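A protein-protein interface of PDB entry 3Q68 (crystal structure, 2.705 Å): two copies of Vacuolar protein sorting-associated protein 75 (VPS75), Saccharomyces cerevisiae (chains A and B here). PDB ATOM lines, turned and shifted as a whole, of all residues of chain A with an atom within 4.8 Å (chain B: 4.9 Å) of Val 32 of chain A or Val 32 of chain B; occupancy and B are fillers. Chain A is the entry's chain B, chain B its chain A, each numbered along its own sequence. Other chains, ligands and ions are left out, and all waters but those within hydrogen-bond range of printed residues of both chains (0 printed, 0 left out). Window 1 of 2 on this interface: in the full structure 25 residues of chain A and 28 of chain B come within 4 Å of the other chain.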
ATOM      1  N   ILE A  28      -0.803  25.330  22.287  1.00  0.00           N
ATOM      2  CA  ILE A  28      -0.625  24.627  21.053  1.00  0.00           C
ATOM      3  C   ILE A  28      -1.063  23.203  21.195  1.00  0.00           C
ATOM      4  O   ILE A  28      -1.673  22.673  20.315  1.00  0.00           O
ATOM      5  CB  ILE A  28       0.824  24.682  20.644  1.00  0.00           C
ATOM      6  CG1 ILE A  28       1.149  26.063  20.148  1.00  0.00           C
ATOM      7  CG2 ILE A  28       1.104  23.755  19.548  1.00  0.00           C
ATOM      8  CD1 ILE A  28       2.495  26.180  19.692  1.00  0.00           C
ATOM      9  N   GLU A  29      -0.782  22.572  22.308  1.00  0.00           N
ATOM     10  CA  GLU A  29      -1.182  21.205  22.445  1.00  0.00           C
ATOM     11  C   GLU A  29      -2.675  21.091  22.345  1.00  0.00           C
ATOM     12  O   GLU A  29      -3.176  20.137  21.798  1.00  0.00           O
ATOM     13  CB  GLU A  29      -0.689  20.653  23.771  1.00  0.00           C
ATOM     14  CG  GLU A  29       0.779  20.307  23.796  1.00  0.00           C
ATOM     15  CD  GLU A  29       1.244  19.930  25.171  1.00  0.00           C
ATOM     16  OE1 GLU A  29       2.432  19.614  25.347  1.00  0.00           O
ATOM     17  OE2 GLU A  29       0.412  19.942  26.090  1.00  0.00           O
ATOM     18  N   ARG A  30      -3.395  22.035  22.917  1.00  0.00           N
ATOM     19  CA  ARG A  30      -4.838  22.020  22.837  1.00  0.00           C
ATOM     20  C   ARG A  30      -5.291  22.205  21.419  1.00  0.00           C
ATOM     21  O   ARG A  30      -6.199  21.562  20.975  1.00  0.00           O
ATOM     22  CB  ARG A  30      -5.453  23.102  23.716  1.00  0.00           C
ATOM     23  CG  ARG A  30      -6.946  22.993  23.842  1.00  0.00           C
ATOM     24  CD  ARG A  30      -7.533  24.108  24.655  1.00  0.00           C
ATOM     25  NE  ARG A  30      -8.944  24.329  24.361  1.00  0.00           N
ATOM     26  CZ  ARG A  30      -9.931  23.612  24.863  1.00  0.00           C
ATOM     27  NH1 ARG A  30      -9.679  22.621  25.688  1.00  0.00           N
ATOM     28  NH2 ARG A  30     -11.166  23.878  24.533  1.00  0.00           N
ATOM     29  N   GLU A  31      -4.656  23.098  20.697  1.00  0.00           N
ATOM     30  CA  GLU A  31      -5.063  23.321  19.333  1.00  0.00           C
ATOM     31  C   GLU A  31      -4.860  22.087  18.508  1.00  0.00           C
ATOM     32  O   GLU A  31      -5.674  21.722  17.701  1.00  0.00           O
ATOM     33  CB  GLU A  31      -4.230  24.404  18.699  1.00  0.00           C
ATOM     34  CG  GLU A  31      -4.485  25.774  19.184  1.00  0.00           C
ATOM     35  CD  GLU A  31      -3.530  26.752  18.583  1.00  0.00           C
ATOM     36  OE1 GLU A  31      -3.855  27.948  18.532  1.00  0.00           O
ATOM     37  OE2 GLU A  31      -2.441  26.325  18.167  1.00  0.00           O
ATOM     38  N   VAL A  32      -3.738  21.443  18.708  1.00  0.00           N
ATOM     39  CA  VAL A  32      -3.429  20.263  17.967  1.00  0.00           C
ATOM     40  C   VAL A  32      -4.409  19.186  18.284  1.00  0.00           C
ATOM     41  O   VAL A  32      -4.838  18.461  17.424  1.00  0.00           O
ATOM     42  CB  VAL A  32      -2.053  19.783  18.301  1.00  0.00           C
ATOM     43  CG1 VAL A  32      -1.860  18.411  17.791  1.00  0.00           C
ATOM     44  CG2 VAL A  32      -1.073  20.701  17.732  1.00  0.00           C
ATOM     45  N   GLU A  33      -4.760  19.072  19.542  1.00  0.00           N
ATOM     46  CA  GLU A  33      -5.651  17.995  19.958  1.00  0.00           C
ATOM     47  C   GLU A  33      -7.055  18.212  19.418  1.00  0.00           C
ATOM     48  O   GLU A  33      -7.718  17.256  19.021  1.00  0.00           O
ATOM     49  CB  GLU A  33      -5.677  17.826  21.478  1.00  0.00           C
ATOM     50  CG  GLU A  33      -6.611  16.724  21.936  1.00  0.00           C
ATOM     51  CD  GLU A  33      -6.280  15.359  21.327  1.00  0.00           C
ATOM     52  OE1 GLU A  33      -5.134  15.176  20.828  1.00  0.00           O
ATOM     53  OE2 GLU A  33      -7.162  14.458  21.361  1.00  0.00           O
ATOM     54  N   LEU A  34      -7.504  19.470  19.419  1.00  0.00           N
ATOM     55  CA  LEU A  34      -8.745  19.845  18.764  1.00  0.00           C
ATOM     56  C   LEU A  34      -8.701  19.498  17.281  1.00  0.00           C
ATOM     57  O   LEU A  34      -9.582  18.803  16.758  1.00  0.00           O
ATOM     58  CB  LEU A  34      -8.990  21.343  18.891  1.00  0.00           C
ATOM     59  CG  LEU A  34      -9.736  21.825  20.130  1.00  0.00           C
ATOM     60  CD1 LEU A  34     -10.240  23.234  19.861  1.00  0.00           C
ATOM     61  CD2 LEU A  34     -10.880  20.895  20.484  1.00  0.00           C
ATOM     62  N   TYR A  35      -7.683  20.021  16.604  1.00  0.00           N
ATOM     63  CA  TYR A  35      -7.472  19.724  15.203  1.00  0.00           C
ATOM     64  C   TYR A  35      -7.678  18.226  14.983  1.00  0.00           C
ATOM     65  O   TYR A  35      -8.423  17.804  14.093  1.00  0.00           O
ATOM     66  CB  TYR A  35      -6.068  20.137  14.816  1.00  0.00           C
ATOM     67  CG  TYR A  35      -5.733  20.004  13.352  1.00  0.00           C
ATOM     68  CD1 TYR A  35      -5.939  21.059  12.476  1.00  0.00           C
ATOM     69  CD2 TYR A  35      -5.163  18.841  12.853  1.00  0.00           C
ATOM     70  CE1 TYR A  35      -5.621  20.952  11.143  1.00  0.00           C
ATOM     71  CE2 TYR A  35      -4.837  18.723  11.527  1.00  0.00           C
ATOM     72  CZ  TYR A  35      -5.071  19.781  10.668  1.00  0.00           C
ATOM     73  OH  TYR A  35      -4.746  19.674   9.326  1.00  0.00           O
ATOM     74  N   ARG A  36      -7.042  17.416  15.814  1.00  0.00           N
ATOM     75  CA  ARG A  36      -7.161  15.991  15.634  1.00  0.00           C
ATOM     76  C   ARG A  36      -8.621  15.549  15.841  1.00  0.00           C
ATOM     77  O   ARG A  36      -9.142  14.743  15.081  1.00  0.00           O
ATOM     78  CB  ARG A  36      -6.182  15.244  16.545  1.00  0.00           C
ATOM     79  CG  ARG A  36      -6.277  13.753  16.439  1.00  0.00           C
ATOM     80  CD  ARG A  36      -5.490  13.044  17.507  1.00  0.00           C
ATOM     81  NE  ARG A  36      -6.284  12.810  18.709  1.00  0.00           N
ATOM     82  CZ  ARG A  36      -7.217  11.863  18.831  1.00  0.00           C
ATOM     83  NH1 ARG A  36      -7.498  11.049  17.814  1.00  0.00           N
ATOM     84  NH2 ARG A  36      -7.885  11.740  19.975  1.00  0.00           N
ATOM     85  N   ILE B  28      -4.700  10.815   9.102  1.00  0.00           N
ATOM     86  CA  ILE B  28      -5.038  11.888   9.999  1.00  0.00           C
ATOM     87  C   ILE B  28      -3.953  12.099  11.018  1.00  0.00           C
ATOM     88  O   ILE B  28      -3.611  13.212  11.331  1.00  0.00           O
ATOM     89  CB  ILE B  28      -6.321  11.589  10.707  1.00  0.00           C
ATOM     90  CG1 ILE B  28      -7.396  11.321   9.688  1.00  0.00           C
ATOM     91  CG2 ILE B  28      -6.758  12.748  11.502  1.00  0.00           C
ATOM     92  CD1 ILE B  28      -8.741  11.503  10.235  1.00  0.00           C
ATOM     93  N   GLU B  29      -3.403  11.025  11.537  1.00  0.00           N
ATOM     94  CA  GLU B  29      -2.369  11.156  12.515  1.00  0.00           C
ATOM     95  C   GLU B  29      -1.193  11.848  11.914  1.00  0.00           C
ATOM     96  O   GLU B  29      -0.604  12.715  12.517  1.00  0.00           O
ATOM     97  CB  GLU B  29      -1.926   9.790  12.984  1.00  0.00           C
ATOM     98  CG  GLU B  29      -2.930   9.045  13.816  1.00  0.00           C
ATOM     99  CD  GLU B  29      -3.339   9.773  15.084  1.00  0.00           C
ATOM    100  OE1 GLU B  29      -2.722  10.792  15.440  1.00  0.00           O
ATOM    101  OE2 GLU B  29      -4.295   9.324  15.735  1.00  0.00           O
ATOM    102  N   ARG B  30      -0.841  11.476  10.705  1.00  0.00           N
ATOM    103  CA  ARG B  30       0.301  12.124  10.104  1.00  0.00           C
ATOM    104  C   ARG B  30       0.064  13.595   9.919  1.00  0.00           C
ATOM    105  O   ARG B  30       0.928  14.418  10.141  1.00  0.00           O
ATOM    106  CB  ARG B  30       0.618  11.508   8.759  1.00  0.00           C
ATOM    107  CG  ARG B  30       1.761  12.211   8.081  1.00  0.00           C
ATOM    108  CD  ARG B  30       1.890  11.891   6.616  1.00  0.00           C
ATOM    109  NE  ARG B  30       2.755  12.859   5.959  1.00  0.00           N
ATOM    110  CZ  ARG B  30       4.076  12.847   6.052  1.00  0.00           C
ATOM    111  NH1 ARG B  30       4.678  11.914   6.774  1.00  0.00           N
ATOM    112  NH2 ARG B  30       4.792  13.767   5.431  1.00  0.00           N
ATOM    113  N   GLU B  31      -1.134  13.925   9.502  1.00  0.00           N
ATOM    114  CA  GLU B  31      -1.493  15.299   9.263  1.00  0.00           C
ATOM    115  C   GLU B  31      -1.381  16.106  10.528  1.00  0.00           C
ATOM    116  O   GLU B  31      -0.899  17.225  10.538  1.00  0.00           O
ATOM    117  CB  GLU B  31      -2.933  15.283   8.836  1.00  0.00           C
ATOM    118  CG  GLU B  31      -3.183  15.064   7.402  1.00  0.00           C
ATOM    119  CD  GLU B  31      -4.641  15.003   7.150  1.00  0.00           C
ATOM    120  OE1 GLU B  31      -5.247  16.076   7.037  1.00  0.00           O
ATOM    121  OE2 GLU B  31      -5.177  13.893   7.035  1.00  0.00           O
ATOM    122  N   VAL B  32      -1.841  15.504  11.604  1.00  0.00           N
ATOM    123  CA  VAL B  32      -1.819  16.113  12.911  1.00  0.00           C
ATOM    124  C   VAL B  32      -0.409  16.359  13.363  1.00  0.00           C
ATOM    125  O   VAL B  32      -0.090  17.397  13.900  1.00  0.00           O
ATOM    126  CB  VAL B  32      -2.478  15.179  13.911  1.00  0.00           C
ATOM    127  CG1 VAL B  32      -2.345  15.693  15.283  1.00  0.00           C
ATOM    128  CG2 VAL B  32      -3.903  14.993  13.570  1.00  0.00           C
ATOM    129  N   GLU B  33       0.449  15.389  13.139  1.00  0.00           N
ATOM    130  CA  GLU B  33       1.819  15.551  13.537  1.00  0.00           C
ATOM    131  C   GLU B  33       2.451  16.671  12.766  1.00  0.00           C
ATOM    132  O   GLU B  33       3.193  17.446  13.300  1.00  0.00           O
ATOM    133  CB  GLU B  33       2.583  14.266  13.349  1.00  0.00           C
ATOM    134  CG  GLU B  33       4.029  14.388  13.669  1.00  0.00           C
ATOM    135  CD  GLU B  33       4.295  14.731  15.098  1.00  0.00           C
ATOM    136  OE1 GLU B  33       3.395  14.583  15.930  1.00  0.00           O
ATOM    137  OE2 GLU B  33       5.421  15.143  15.395  1.00  0.00           O
ATOM    138  N   LEU B  34       2.152  16.766  11.492  1.00  0.00           N
ATOM    139  CA  LEU B  34       2.729  17.833  10.719  1.00  0.00           C
ATOM    140  C   LEU B  34       2.265  19.159  11.213  1.00  0.00           C
ATOM    141  O   LEU B  34       3.003  20.117  11.239  1.00  0.00           O
ATOM    142  CB  LEU B  34       2.344  17.698   9.273  1.00  0.00           C
ATOM    143  CG  LEU B  34       3.460  17.205   8.392  1.00  0.00           C
ATOM    144  CD1 LEU B  34       2.944  17.205   7.020  1.00  0.00           C
ATOM    145  CD2 LEU B  34       4.623  18.118   8.500  1.00  0.00           C
ATOM    146  N   TYR B  35       1.007  19.211  11.586  1.00  0.00           N
ATOM    147  CA  TYR B  35       0.416  20.422  12.086  1.00  0.00           C
ATOM    148  C   TYR B  35       1.118  20.847  13.348  1.00  0.00           C
ATOM    149  O   TYR B  35       1.412  22.010  13.507  1.00  0.00           O
ATOM    150  CB  TYR B  35      -1.054  20.155  12.351  1.00  0.00           C
ATOM    151  CG  TYR B  35      -1.864  21.325  12.809  1.00  0.00           C
ATOM    152  CD1 TYR B  35      -2.292  22.276  11.929  1.00  0.00           C
ATOM    153  CD2 TYR B  35      -2.230  21.450  14.121  1.00  0.00           C
ATOM    154  CE1 TYR B  35      -3.028  23.327  12.348  1.00  0.00           C
ATOM    155  CE2 TYR B  35      -2.963  22.486  14.541  1.00  0.00           C
ATOM    156  CZ  TYR B  35      -3.368  23.420  13.658  1.00  0.00           C
ATOM    157  OH  TYR B  35      -4.113  24.467  14.110  1.00  0.00           O
ATOM    158  N   ARG B  36       1.400  19.904  14.238  1.00  0.00           N
ATOM    159  CA  ARG B  36       2.085  20.232  15.477  1.00  0.00           C
ATOM    160  C   ARG B  36       3.477  20.743  15.229  1.00  0.00           C
ATOM    161  O   ARG B  36       3.879  21.744  15.753  1.00  0.00           O
ATOM    162  CB  ARG B  36       2.163  19.001  16.345  1.00  0.00           C
ATOM    163  CG  ARG B  36       2.532  19.283  17.750  1.00  0.00           C
ATOM    164  CD  ARG B  36       2.495  18.042  18.555  1.00  0.00           C
ATOM    165  NE  ARG B  36       3.348  17.051  17.958  1.00  0.00           N
ATOM    166  CZ  ARG B  36       4.664  17.044  18.078  1.00  0.00           C
ATOM    167  NH1 ARG B  36       5.268  17.977  18.781  1.00  0.00           N
ATOM    168  NH2 ARG B  36       5.375  16.104  17.484  1.00  0.00           N
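Among the printed residues, merely in contact across the chains: Val 32 of chain A with Val 32 of chain B (3.7 Å), Val 32 of chain A with Tyr 35 of chain B (3.9 Å), Val 32 of chain A with Arg 36 of chain B (3.9 Å), Tyr 35 of chain A with Tyr 35 of chain B (3.7 Å) and Arg 36 of chain A with Val 32 of chain B (3.8 Å).
Hydrophobic or aromatic side chains of chain A within 4 Å of the printed part of chain B: Val 32 and Tyr 35.
Of the 9 printed residues of chain B, 3 touch a printed residue of chain A.
Among the printed residues, 5 pairs touch across the chains.
Among the printed residues, no Asp or Glu carboxylate lies within 4 Å of a Lys or Arg side-chain nitrogen of the other chain.
Ile 28 of chain A touches none of the printed residues of chain B.
Of chain B, only Val 32 (3.7 Å), Tyr 35 (3.9 Å) and Arg 36 (3.9 Å) come within 4 Å of Val 32 of chain A.
Printed residues of chain B within 4 Å of Tyr 35 of chain A: Tyr 35 (3.7 Å).
Printed residues of chain B within 4 Å of Arg 36 of chain A: Val 32.
Ile 28 of chain B touches none of the printed residues of chain A.
Val 32 of chain B touches just these residues of chain A: Val 32 and Arg 36.
Printed residues of chain A within 4 Å of Tyr 35 of chain B: Val 32 and Tyr 35.
Of the printed residues of chain A, Arg 36 of chain B touches Val 32.
The nearest printed residue of chain B that does not touch Val 32 of chain A is Glu 33 of chain B (6.0 Å).
The side-chain carboxylate (OE1) of Glu 33 of chain B is in salt-bridge range of the guanidinium group (NH2) of Arg 36 of chain B, at 2.9 Å.
The guanidinium group (NH2) of Arg 36 of chain A lies within salt-bridge range of the side-chain carboxylate (OE2) of Glu 33 of chain A, 3.1 Å away.
Val 32 of chain B touches its own counterpart, Val 32 of chain A.
Val 32 of chain A touches Tyr 35 of chain B, but with the chains exchanged Tyr 35 of chain A does not touch Val 32 of chain B (4.1 Å).
Val 32 of chain A touches Arg 36 of chain B, and with the chains exchanged Arg 36 of chain A touches Val 32 of chain B.
Tyr 35 of chain B touches its own counterpart, Tyr 35 of chain A.
Positions printed for both chains: 28, 29, 30, 31, 32, 33, 34, 35 and 36.
Of the 5 pairs that touch across the chains among the printed residues, 4 have their exchanged pair printed and touching as well.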
